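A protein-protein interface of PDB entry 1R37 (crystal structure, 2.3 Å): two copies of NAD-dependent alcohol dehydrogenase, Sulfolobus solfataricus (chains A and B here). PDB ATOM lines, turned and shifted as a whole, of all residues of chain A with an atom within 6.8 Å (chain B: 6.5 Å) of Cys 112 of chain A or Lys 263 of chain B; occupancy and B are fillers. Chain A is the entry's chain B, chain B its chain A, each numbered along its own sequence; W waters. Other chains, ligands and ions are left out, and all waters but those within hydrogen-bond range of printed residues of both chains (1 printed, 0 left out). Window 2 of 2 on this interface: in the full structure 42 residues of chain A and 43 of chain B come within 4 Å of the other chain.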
ATOM      1  N   GLN A  96     -12.920   9.071 -12.475  1.00  0.00           N
ATOM      2  CA  GLN A  96     -11.947   8.246 -11.778  1.00  0.00           C
ATOM      3  C   GLN A  96     -12.386   7.509 -10.527  1.00  0.00           C
ATOM      4  O   GLN A  96     -13.170   8.017  -9.722  1.00  0.00           O
ATOM      5  CB  GLN A  96     -10.719   9.105 -11.490  1.00  0.00           C
ATOM      6  CG  GLN A  96     -10.137   9.649 -12.777  1.00  0.00           C
ATOM      7  CD  GLN A  96      -8.899  10.486 -12.580  1.00  0.00           C
ATOM      8  OE1 GLN A  96      -8.082  10.208 -11.701  1.00  0.00           O
ATOM      9  NE2 GLN A  96      -8.737  11.504 -13.420  1.00  0.00           N
ATOM     10  N   GLY A  97     -11.868   6.291 -10.390  1.00  0.00           N
ATOM     11  CA  GLY A  97     -12.169   5.465  -9.238  1.00  0.00           C
ATOM     12  C   GLY A  97     -10.910   5.223  -8.427  1.00  0.00           C
ATOM     13  O   GLY A  97      -9.799   5.338  -8.946  1.00  0.00           O
ATOM     14  N   GLU A  98     -11.078   4.877  -7.156  1.00  0.00           N
ATOM     15  CA  GLU A  98      -9.946   4.650  -6.267  1.00  0.00           C
ATOM     16  C   GLU A  98      -9.214   3.320  -6.475  1.00  0.00           C
ATOM     17  O   GLU A  98      -8.094   3.154  -5.992  1.00  0.00           O
ATOM     18  CB  GLU A  98     -10.403   4.801  -4.814  1.00  0.00           C
ATOM     19  CG  GLU A  98     -11.680   4.044  -4.468  1.00  0.00           C
ATOM     20  CD  GLU A  98     -11.489   2.543  -4.450  1.00  0.00           C
ATOM     21  OE1 GLU A  98     -10.470   2.088  -3.890  1.00  0.00           O
ATOM     22  OE2 GLU A  98     -12.357   1.807  -4.966  1.00  0.00           O
ATOM     23  N   GLY A  99      -9.844   2.378  -7.179  1.00  0.00           N
ATOM     24  CA  GLY A  99      -9.193   1.115  -7.499  1.00  0.00           C
ATOM     25  C   GLY A  99      -9.393  -0.139  -6.654  1.00  0.00           C
ATOM     26  O   GLY A  99      -8.992  -1.224  -7.079  1.00  0.00           O
ATOM     27  N   ASN A 100     -10.015  -0.019  -5.484  1.00  0.00           N
ATOM     28  CA  ASN A 100     -10.180  -1.168  -4.594  1.00  0.00           C
ATOM     29  C   ASN A 100     -11.608  -1.684  -4.391  1.00  0.00           C
ATOM     30  O   ASN A 100     -11.792  -2.846  -4.023  1.00  0.00           O
ATOM     31  CB  ASN A 100      -9.554  -0.846  -3.229  1.00  0.00           C
ATOM     32  CG  ASN A 100      -9.584  -2.026  -2.271  1.00  0.00           C
ATOM     33  OD1 ASN A 100      -9.032  -3.093  -2.555  1.00  0.00           O
ATOM     34  ND2 ASN A 100     -10.220  -1.835  -1.121  1.00  0.00           N
ATOM     35  N   CYS A 101     -12.613  -0.839  -4.621  1.00  0.00           N
ATOM     36  CA  CYS A 101     -14.006  -1.259  -4.433  1.00  0.00           C
ATOM     37  C   CYS A 101     -14.419  -2.268  -5.498  1.00  0.00           C
ATOM     38  O   CYS A 101     -13.710  -2.472  -6.483  1.00  0.00           O
ATOM     39  CB  CYS A 101     -14.953  -0.059  -4.495  1.00  0.00           C
ATOM     40  SG  CYS A 101     -15.235   0.589  -6.175  1.00  0.00           S
ATOM     41  N   TYR A 102     -15.574  -2.892  -5.284  1.00  0.00           N
ATOM     42  CA  TYR A 102     -16.125  -3.882  -6.199  1.00  0.00           C
ATOM     43  C   TYR A 102     -16.163  -3.403  -7.648  1.00  0.00           C
ATOM     44  O   TYR A 102     -15.707  -4.100  -8.550  1.00  0.00           O
ATOM     45  CB  TYR A 102     -17.546  -4.255  -5.771  1.00  0.00           C
ATOM     46  CG  TYR A 102     -18.225  -5.222  -6.714  1.00  0.00           C
ATOM     47  CD1 TYR A 102     -17.925  -6.586  -6.679  1.00  0.00           C
ATOM     48  CD2 TYR A 102     -19.134  -4.770  -7.672  1.00  0.00           C
ATOM     49  CE1 TYR A 102     -18.514  -7.480  -7.579  1.00  0.00           C
ATOM     50  CE2 TYR A 102     -19.724  -5.650  -8.576  1.00  0.00           C
ATOM     51  CZ  TYR A 102     -19.408  -7.004  -8.522  1.00  0.00           C
ATOM     52  OH  TYR A 102     -19.972  -7.881  -9.422  1.00  0.00           O
ATOM     53  N   TYR A 103     -16.710  -2.216  -7.871  1.00  0.00           N
ATOM     54  CA  TYR A 103     -16.839  -1.698  -9.226  1.00  0.00           C
ATOM     55  C   TYR A 103     -15.503  -1.407  -9.901  1.00  0.00           C
ATOM     56  O   TYR A 103     -15.358  -1.611 -11.105  1.00  0.00           O
ATOM     57  CB  TYR A 103     -17.768  -0.477  -9.217  1.00  0.00           C
ATOM     58  CG  TYR A 103     -19.197  -0.880  -8.872  1.00  0.00           C
ATOM     59  CD1 TYR A 103     -20.019  -1.488  -9.822  1.00  0.00           C
ATOM     60  CD2 TYR A 103     -19.676  -0.774  -7.566  1.00  0.00           C
ATOM     61  CE1 TYR A 103     -21.279  -1.994  -9.479  1.00  0.00           C
ATOM     62  CE2 TYR A 103     -20.931  -1.272  -7.211  1.00  0.00           C
ATOM     63  CZ  TYR A 103     -21.728  -1.885  -8.170  1.00  0.00           C
ATOM     64  OH  TYR A 103     -22.963  -2.388  -7.813  1.00  0.00           O
ATOM     65  N   CYS A 104     -14.517  -0.953  -9.136  1.00  0.00           N
ATOM     66  CA  CYS A 104     -13.199  -0.716  -9.713  1.00  0.00           C
ATOM     67  C   CYS A 104     -12.556  -2.051 -10.097  1.00  0.00           C
ATOM     68  O   CYS A 104     -11.898  -2.150 -11.125  1.00  0.00           O
ATOM     69  CB  CYS A 104     -12.289   0.028  -8.728  1.00  0.00           C
ATOM     70  SG  CYS A 104     -12.572   1.829  -8.621  1.00  0.00           S
ATOM     71  N   GLU A 108     -15.208  -1.229 -13.866  1.00  0.00           N
ATOM     72  CA  GLU A 108     -16.286  -0.249 -14.018  1.00  0.00           C
ATOM     73  C   GLU A 108     -15.940   0.933 -13.108  1.00  0.00           C
ATOM     74  O   GLU A 108     -16.744   1.360 -12.270  1.00  0.00           O
ATOM     75  CB  GLU A 108     -17.629  -0.869 -13.603  1.00  0.00           C
ATOM     76  CG  GLU A 108     -18.062  -2.107 -14.419  1.00  0.00           C
ATOM     77  CD  GLU A 108     -18.306  -1.810 -15.901  1.00  0.00           C
ATOM     78  OE1 GLU A 108     -18.697  -0.671 -16.229  1.00  0.00           O
ATOM     79  OE2 GLU A 108     -18.124  -2.718 -16.744  1.00  0.00           O
ATOM     80  N   GLU A 109     -14.728   1.459 -13.283  1.00  0.00           N
ATOM     81  CA  GLU A 109     -14.244   2.531 -12.427  1.00  0.00           C
ATOM     82  C   GLU A 109     -15.117   3.767 -12.293  1.00  0.00           C
ATOM     83  O   GLU A 109     -15.039   4.457 -11.277  1.00  0.00           O
ATOM     84  CB  GLU A 109     -12.813   2.944 -12.811  1.00  0.00           C
ATOM     85  CG  GLU A 109     -12.415   2.718 -14.247  1.00  0.00           C
ATOM     86  CD  GLU A 109     -11.844   1.339 -14.496  1.00  0.00           C
ATOM     87  OE1 GLU A 109     -10.853   0.970 -13.831  1.00  0.00           O
ATOM     88  OE2 GLU A 109     -12.386   0.632 -15.365  1.00  0.00           O
ATOM     89  N   HIS A 110     -15.956   4.055 -13.284  1.00  0.00           N
ATOM     90  CA  HIS A 110     -16.816   5.230 -13.178  1.00  0.00           C
ATOM     91  C   HIS A 110     -17.933   5.018 -12.151  1.00  0.00           C
ATOM     92  O   HIS A 110     -18.562   5.977 -11.699  1.00  0.00           O
ATOM     93  CB  HIS A 110     -17.417   5.583 -14.534  1.00  0.00           C
ATOM     94  CG  HIS A 110     -18.271   4.504 -15.116  1.00  0.00           C
ATOM     95  ND1 HIS A 110     -17.771   3.269 -15.467  1.00  0.00           N
ATOM     96  CD2 HIS A 110     -19.588   4.484 -15.431  1.00  0.00           C
ATOM     97  CE1 HIS A 110     -18.743   2.533 -15.976  1.00  0.00           C
ATOM     98  NE2 HIS A 110     -19.855   3.246 -15.966  1.00  0.00           N
ATOM     99  N   LEU A 111     -18.169   3.762 -11.781  1.00  0.00           N
ATOM    100  CA  LEU A 111     -19.199   3.428 -10.799  1.00  0.00           C
ATOM    101  C   LEU A 111     -18.574   3.132  -9.438  1.00  0.00           C
ATOM    102  O   LEU A 111     -19.152   2.436  -8.594  1.00  0.00           O
ATOM    103  CB  LEU A 111     -20.019   2.229 -11.276  1.00  0.00           C
ATOM    104  CG  LEU A 111     -20.870   2.492 -12.518  1.00  0.00           C
ATOM    105  CD1 LEU A 111     -21.589   1.222 -12.921  1.00  0.00           C
ATOM    106  CD2 LEU A 111     -21.874   3.604 -12.231  1.00  0.00           C
ATOM    107  N   CYS A 112     -17.383   3.675  -9.236  1.00  0.00           N
ATOM    108  CA  CYS A 112     -16.663   3.527  -7.979  1.00  0.00           C
ATOM    109  C   CYS A 112     -17.501   4.001  -6.788  1.00  0.00           C
ATOM    110  O   CYS A 112     -18.284   4.951  -6.913  1.00  0.00           O
ATOM    111  CB  CYS A 112     -15.371   4.336  -8.039  1.00  0.00           C
ATOM    112  SG  CYS A 112     -14.426   4.284  -6.493  1.00  0.00           S
ATOM    113  N   ASP A 113     -17.331   3.342  -5.639  1.00  0.00           N
ATOM    114  CA  ASP A 113     -18.064   3.713  -4.424  1.00  0.00           C
ATOM    115  C   ASP A 113     -17.574   5.053  -3.864  1.00  0.00           C
ATOM    116  O   ASP A 113     -18.299   5.735  -3.134  1.00  0.00           O
ATOM    117  CB  ASP A 113     -17.920   2.634  -3.336  1.00  0.00           C
ATOM    118  CG  ASP A 113     -18.652   1.346  -3.677  1.00  0.00           C
ATOM    119  OD1 ASP A 113     -19.744   1.411  -4.287  1.00  0.00           O
ATOM    120  OD2 ASP A 113     -18.138   0.265  -3.317  1.00  0.00           O
ATOM    121  N   SER A 114     -16.337   5.415  -4.195  1.00  0.00           N
ATOM    122  CA  SER A 114     -15.745   6.685  -3.765  1.00  0.00           C
ATOM    123  C   SER A 114     -15.218   7.382  -5.012  1.00  0.00           C
ATOM    124  O   SER A 114     -14.015   7.585  -5.167  1.00  0.00           O
ATOM    125  CB  SER A 114     -14.601   6.443  -2.780  1.00  0.00           C
ATOM    126  OG  SER A 114     -15.080   5.827  -1.598  1.00  0.00           O
ATOM    127  N   PRO A 115     -16.133   7.775  -5.913  1.00  0.00           N
ATOM    128  CA  PRO A 115     -15.790   8.437  -7.172  1.00  0.00           C
ATOM    129  C   PRO A 115     -15.110   9.795  -7.067  1.00  0.00           C
ATOM    130  O   PRO A 115     -15.414  10.600  -6.187  1.00  0.00           O
ATOM    131  CB  PRO A 115     -17.136   8.521  -7.885  1.00  0.00           C
ATOM    132  CG  PRO A 115     -18.077   8.755  -6.754  1.00  0.00           C
ATOM    133  CD  PRO A 115     -17.596   7.768  -5.710  1.00  0.00           C
ATOM    134  N   ARG A 116     -14.176  10.024  -7.983  1.00  0.00           N
ATOM    135  CA  ARG A 116     -13.479  11.293  -8.088  1.00  0.00           C
ATOM    136  C   ARG A 116     -13.763  11.754  -9.512  1.00  0.00           C
ATOM    137  O   ARG A 116     -13.066  11.368 -10.454  1.00  0.00           O
ATOM    138  CB  ARG A 116     -11.977  11.098  -7.868  1.00  0.00           C
ATOM    139  CG  ARG A 116     -11.624  10.625  -6.463  1.00  0.00           C
ATOM    140  CD  ARG A 116     -10.205  10.094  -6.406  1.00  0.00           C
ATOM    141  NE  ARG A 116      -9.879   9.490  -5.115  1.00  0.00           N
ATOM    142  CZ  ARG A 116      -8.770   8.790  -4.882  1.00  0.00           C
ATOM    143  NH1 ARG A 116      -7.879   8.604  -5.855  1.00  0.00           N
ATOM    144  NH2 ARG A 116      -8.547   8.272  -3.679  1.00  0.00           N
ATOM    145  N   TRP A 117     -14.812  12.553  -9.662  1.00  0.00           N
ATOM    146  CA  TRP A 117     -15.228  13.040 -10.967  1.00  0.00           C
ATOM    147  C   TRP A 117     -14.841  14.490 -11.167  1.00  0.00           C
ATOM    148  O   TRP A 117     -15.504  15.402 -10.649  1.00  0.00           O
ATOM    149  CB  TRP A 117     -16.745  12.910 -11.134  1.00  0.00           C
ATOM    150  CG  TRP A 117     -17.253  11.500 -11.202  1.00  0.00           C
ATOM    151  CD1 TRP A 117     -16.518  10.353 -11.125  1.00  0.00           C
ATOM    152  CD2 TRP A 117     -18.614  11.094 -11.370  1.00  0.00           C
ATOM    153  NE1 TRP A 117     -17.338   9.254 -11.236  1.00  0.00           N
ATOM    154  CE2 TRP A 117     -18.631   9.682 -11.388  1.00  0.00           C
ATOM    155  CE3 TRP A 117     -19.825  11.791 -11.510  1.00  0.00           C
ATOM    156  CZ2 TRP A 117     -19.813   8.946 -11.542  1.00  0.00           C
ATOM    157  CZ3 TRP A 117     -21.004  11.060 -11.666  1.00  0.00           C
ATOM    158  CH2 TRP A 117     -20.986   9.649 -11.679  1.00  0.00           C
ATOM    159  N   TYR A 137      -5.308   7.529 -15.879  1.00  0.00           N
ATOM    160  CA  TYR A 137      -6.541   7.952 -16.544  1.00  0.00           C
ATOM    161  C   TYR A 137      -6.279   8.952 -17.661  1.00  0.00           C
ATOM    162  O   TYR A 137      -7.194   9.654 -18.099  1.00  0.00           O
ATOM    163  CB  TYR A 137      -7.505   8.584 -15.534  1.00  0.00           C
ATOM    164  CG  TYR A 137      -8.196   7.590 -14.631  1.00  0.00           C
ATOM    165  CD1 TYR A 137      -9.334   6.901 -15.057  1.00  0.00           C
ATOM    166  CD2 TYR A 137      -7.709   7.335 -13.351  1.00  0.00           C
ATOM    167  CE1 TYR A 137      -9.972   5.986 -14.231  1.00  0.00           C
ATOM    168  CE2 TYR A 137      -8.335   6.422 -12.515  1.00  0.00           C
ATOM    169  CZ  TYR A 137      -9.467   5.750 -12.959  1.00  0.00           C
ATOM    170  OH  TYR A 137     -10.087   4.849 -12.124  1.00  0.00           O
ATOM    171  N   LYS B 239     -25.243  -2.786  -0.274  1.00  0.00           N
ATOM    172  CA  LYS B 239     -24.885  -2.741  -1.688  1.00  0.00           C
ATOM    173  C   LYS B 239     -26.122  -2.863  -2.567  1.00  0.00           C
ATOM    174  O   LYS B 239     -26.168  -2.304  -3.665  1.00  0.00           O
ATOM    175  CB  LYS B 239     -23.914  -3.865  -2.057  1.00  0.00           C
ATOM    176  CG  LYS B 239     -23.492  -3.833  -3.532  1.00  0.00           C
ATOM    177  CD  LYS B 239     -22.820  -5.130  -3.973  1.00  0.00           C
ATOM    178  CE  LYS B 239     -22.621  -5.152  -5.485  1.00  0.00           C
ATOM    179  NZ  LYS B 239     -22.152  -6.483  -5.977  1.00  0.00           N
ATOM    180  N   VAL B 241     -29.154  -5.490  -4.427  1.00  0.00           N
ATOM    181  CA  VAL B 241     -29.015  -6.698  -5.235  1.00  0.00           C
ATOM    182  C   VAL B 241     -28.623  -6.401  -6.678  1.00  0.00           C
ATOM    183  O   VAL B 241     -29.049  -5.410  -7.264  1.00  0.00           O
ATOM    184  CB  VAL B 241     -30.305  -7.548  -5.238  1.00  0.00           C
ATOM    185  CG1 VAL B 241     -30.606  -8.036  -3.825  1.00  0.00           C
ATOM    186  CG2 VAL B 241     -31.470  -6.749  -5.820  1.00  0.00           C
ATOM    187  N   ASP B 242     -27.815  -7.289  -7.244  1.00  0.00           N
ATOM    188  CA  ASP B 242     -27.326  -7.139  -8.606  1.00  0.00           C
ATOM    189  C   ASP B 242     -28.383  -7.498  -9.628  1.00  0.00           C
ATOM    190  O   ASP B 242     -28.291  -7.109 -10.793  1.00  0.00           O
ATOM    191  CB  ASP B 242     -26.086  -8.013  -8.801  1.00  0.00           C
ATOM    192  CG  ASP B 242     -24.980  -7.655  -7.837  1.00  0.00           C
ATOM    193  OD1 ASP B 242     -24.329  -6.611  -8.045  1.00  0.00           O
ATOM    194  OD2 ASP B 242     -24.774  -8.406  -6.857  1.00  0.00           O
ATOM    195  N   LEU B 261     -32.046  -2.260  -5.911  1.00  0.00           N
ATOM    196  CA  LEU B 261     -31.029  -2.546  -6.919  1.00  0.00           C
ATOM    197  C   LEU B 261     -29.693  -1.881  -6.644  1.00  0.00           C
ATOM    198  O   LEU B 261     -29.636  -0.729  -6.217  1.00  0.00           O
ATOM    199  CB  LEU B 261     -31.505  -2.095  -8.307  1.00  0.00           C
ATOM    200  CG  LEU B 261     -32.591  -2.880  -9.036  1.00  0.00           C
ATOM    201  CD1 LEU B 261     -32.953  -2.160 -10.322  1.00  0.00           C
ATOM    202  CD2 LEU B 261     -32.097  -4.291  -9.334  1.00  0.00           C
ATOM    203  N   ALA B 262     -28.615  -2.616  -6.904  1.00  0.00           N
ATOM    204  CA  ALA B 262     -27.268  -2.084  -6.751  1.00  0.00           C
ATOM    205  C   ALA B 262     -26.972  -1.329  -8.038  1.00  0.00           C
ATOM    206  O   ALA B 262     -27.778  -1.350  -8.967  1.00  0.00           O
ATOM    207  CB  ALA B 262     -26.278  -3.224  -6.589  1.00  0.00           C
ATOM    208  N   LYS B 263     -25.835  -0.650  -8.105  1.00  0.00           N
ATOM    209  CA  LYS B 263     -25.454  -0.005  -9.352  1.00  0.00           C
ATOM    210  C   LYS B 263     -25.278  -1.138 -10.379  1.00  0.00           C
ATOM    211  O   LYS B 263     -24.776  -2.218 -10.039  1.00  0.00           O
ATOM    212  CB  LYS B 263     -24.155   0.782  -9.166  1.00  0.00           C
ATOM    213  CG  LYS B 263     -24.350   2.096  -8.413  1.00  0.00           C
ATOM    214  CD  LYS B 263     -23.019   2.787  -8.091  1.00  0.00           C
ATOM    215  CE  LYS B 263     -22.233   2.021  -7.025  1.00  0.00           C
ATOM    216  NZ  LYS B 263     -20.948   2.705  -6.636  1.00  0.00           N
ATOM    217  N   GLN B 264     -25.713  -0.884 -11.613  1.00  0.00           N
ATOM    218  CA  GLN B 264     -25.694  -1.856 -12.716  1.00  0.00           C
ATOM    219  C   GLN B 264     -26.716  -2.986 -12.544  1.00  0.00           C
ATOM    220  O   GLN B 264     -26.735  -3.939 -13.322  1.00  0.00           O
ATOM    221  CB  GLN B 264     -24.295  -2.470 -12.896  1.00  0.00           C
ATOM    222  CG  GLN B 264     -23.266  -1.530 -13.501  1.00  0.00           C
ATOM    223  CD  GLN B 264     -22.009  -2.263 -13.942  1.00  0.00           C
ATOM    224  OE1 GLN B 264     -21.429  -3.044 -13.182  1.00  0.00           O
ATOM    225  NE2 GLN B 264     -21.579  -2.014 -15.174  1.00  0.00           N
ATOM    226  N   GLY B 265     -27.565  -2.877 -11.530  1.00  0.00           N
ATOM    227  CA  GLY B 265     -28.554  -3.915 -11.283  1.00  0.00           C
ATOM    228  C   GLY B 265     -29.533  -4.156 -12.415  1.00  0.00           C
ATOM    229  O   GLY B 265     -29.968  -3.223 -13.087  1.00  0.00           O
ATOM    230  N   LEU B 286     -27.918   7.453 -13.697  1.00  0.00           N
ATOM    231  CA  LEU B 286     -26.822   7.557 -12.741  1.00  0.00           C
ATOM    232  C   LEU B 286     -26.388   6.235 -12.084  1.00  0.00           C
ATOM    233  O   LEU B 286     -25.238   6.093 -11.666  1.00  0.00           O
ATOM    234  CB  LEU B 286     -27.190   8.577 -11.665  1.00  0.00           C
ATOM    235  CG  LEU B 286     -27.587   9.945 -12.228  1.00  0.00           C
ATOM    236  CD1 LEU B 286     -28.001  10.866 -11.087  1.00  0.00           C
ATOM    237  CD2 LEU B 286     -26.429  10.544 -13.024  1.00  0.00           C
ATOM    238  N   SER B 287     -27.301   5.272 -11.994  1.00  0.00           N
ATOM    239  CA  SER B 287     -26.982   3.980 -11.389  1.00  0.00           C
ATOM    240  C   SER B 287     -26.767   2.901 -12.441  1.00  0.00           C
ATOM    241  O   SER B 287     -26.402   1.781 -12.104  1.00  0.00           O
ATOM    242  CB  SER B 287     -28.115   3.516 -10.473  1.00  0.00           C
ATOM    243  OG  SER B 287     -28.395   4.451  -9.458  1.00  0.00           O
ATOM    244  N   GLU B 288     -27.005   3.247 -13.705  1.00  0.00           N
ATOM    245  CA  GLU B 288     -26.908   2.301 -14.819  1.00  0.00           C
ATOM    246  C   GLU B 288     -27.759   1.055 -14.599  1.00  0.00           C
ATOM    247  O   GLU B 288     -27.358  -0.045 -14.995  1.00  0.00           O
ATOM    248  CB  GLU B 288     -25.460   1.850 -15.067  1.00  0.00           C
ATOM    249  CG  GLU B 288     -24.542   2.908 -15.654  1.00  0.00           C
ATOM    250  CD  GLU B 288     -23.378   2.293 -16.417  1.00  0.00           C
ATOM    251  OE1 GLU B 288     -22.931   1.190 -16.037  1.00  0.00           O
ATOM    252  OE2 GLU B 288     -22.907   2.908 -17.396  1.00  0.00           O
ATOM    253  N   ILE B 289     -28.922   1.203 -13.968  1.00  0.00           N
ATOM    254  CA  ILE B 289     -29.769   0.033 -13.779  1.00  0.00           C
ATOM    255  C   ILE B 289     -30.508  -0.215 -15.078  1.00  0.00           C
ATOM    256  O   ILE B 289     -30.558   0.661 -15.944  1.00  0.00           O
ATOM    257  CB  ILE B 289     -30.804   0.199 -12.623  1.00  0.00           C
ATOM    258  CG1 ILE B 289     -31.694   1.409 -12.865  1.00  0.00           C
ATOM    259  CG2 ILE B 289     -30.083   0.300 -11.280  1.00  0.00           C
ATOM    260  CD1 ILE B 289     -32.709   1.635 -11.747  1.00  0.00           C
HETATM  261  O   HOH W   1     -24.217  -0.519  -5.412  1.00  0.00           O
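Of the printed residues of chain B, Tyr 102 of chain A touches Lys 239.
Printed residues of chain B within 4 Å of Leu 111 of chain A: Lys 263 (2.7 Å), Gln 264 (3.3 Å) and Glu 288 (3.4 Å).
Of chain B, only Lys 263 comes within 4 Å of Cys 112 of chain A.
Printed residues of chain B within 4 Å of Asp 113 of chain A: Lys 263.
Lys 263 of chain B touches just these residues of chain A: Tyr 103 (2.9 Å), Leu 111 (2.7 Å), Cys 112 (3.5 Å) and Asp 113 (2.9 Å).
Of the printed residues of chain A, Glu 288 of chain B touches His 110 (3.4 Å) and Leu 111 (3.4 Å).
The nearest printed residue of chain B that does not touch Cys 112 of chain A is Leu 286 of chain B (8.5 Å).
The nearest printed residue of chain B that does not touch Asp 113 of chain A is Lys 239 of chain B (6.5 Å).
Among the printed residues, merely in contact across the chains: Leu 111 of chain A with Gln 264 of chain B (3.3 Å), Leu 111 of chain A with Glu 288 of chain B (3.4 Å), Tyr 103 of chain A with Lys 239 of chain B (3.6 Å), Tyr 103 of chain A with Ala 262 of chain B (3.6 Å), Tyr 102 of chain A with Lys 239 of chain B (3.7 Å) and Tyr 103 of chain A with Gln 264 of chain B (3.9 Å).
Printed residues of chain B that touch a printed residue of chain A: Lys 239, Ala 262, Lys 263, Gln 264 and Glu 288.
Among the printed residues, 12 pairs touch across the chains.
Among the printed residues, Asp or Glu carboxylates within 4 Å of a Lys or Arg side-chain nitrogen of the other chain: Asp 113 of chain A with Lys 263 of chain B.
Water W1 lies within hydrogen-bond range of N of Lys 263 of chain B, O of Lys 239 of chain B and OH of Tyr 103 of chain A.
No position is printed for both chains.
Of the 12 pairs that touch across the chains among the printed residues, none has its exchanged pair printed and touching as well.
The backbone carbonyl oxygen of Val 241 of chain B is in hydrogen-bond range of the backbone NH of Ala 262 of chain B, 2.9 Å away.
O of Ser 287 of chain B is in hydrogen-bond range of N of Gln 264 of chain B, at 2.8 Å.
SG of Cys 101 of chain A sits close to N of Tyr 103 of chain A, at 3.6 Å.
The side-chain sulfur (SG) of Cys 101 of chain A lies close to the backbone NH (N) of Asp 113 of chain A (3.5 Å).
The backbone NH (N) of Glu 108 of chain A is in hydrogen-bond range of the backbone carbonyl oxygen (O) of Tyr 103 of chain A, at 2.8 Å.
The side-chain sulfur (SG) of Cys 112 of chain A sits close to the backbone NH (N) of Ser 114 of chain A (3.2 Å).
The backbone carbonyl oxygen (O) of Lys 263 of chain B is in hydrogen-bond range of the side-chain hydroxyl (OH) of Tyr 103 of chain A (2.9 Å).
O of Leu 111 of chain A is in hydrogen-bond range of NZ of Lys 263 of chain B (2.7 Å).
NZ of Lys 263 of chain B is in hydrogen-bond range of O of Cys 112 of chain A.
The side-chain amino group (NZ) of Lys 263 of chain B is in salt-bridge range of the side-chain carboxylate (OD1) of Asp 113 of chain A (2.9 Å).
NE2 of Gln 264 of chain B sits at hydrogen-bond distance from OE1 of Glu 108 of chain A, 3.4 Å away.
OE2 of Glu 288 of chain B is in hydrogen-bond range of NE2 of His 110 of chain A.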
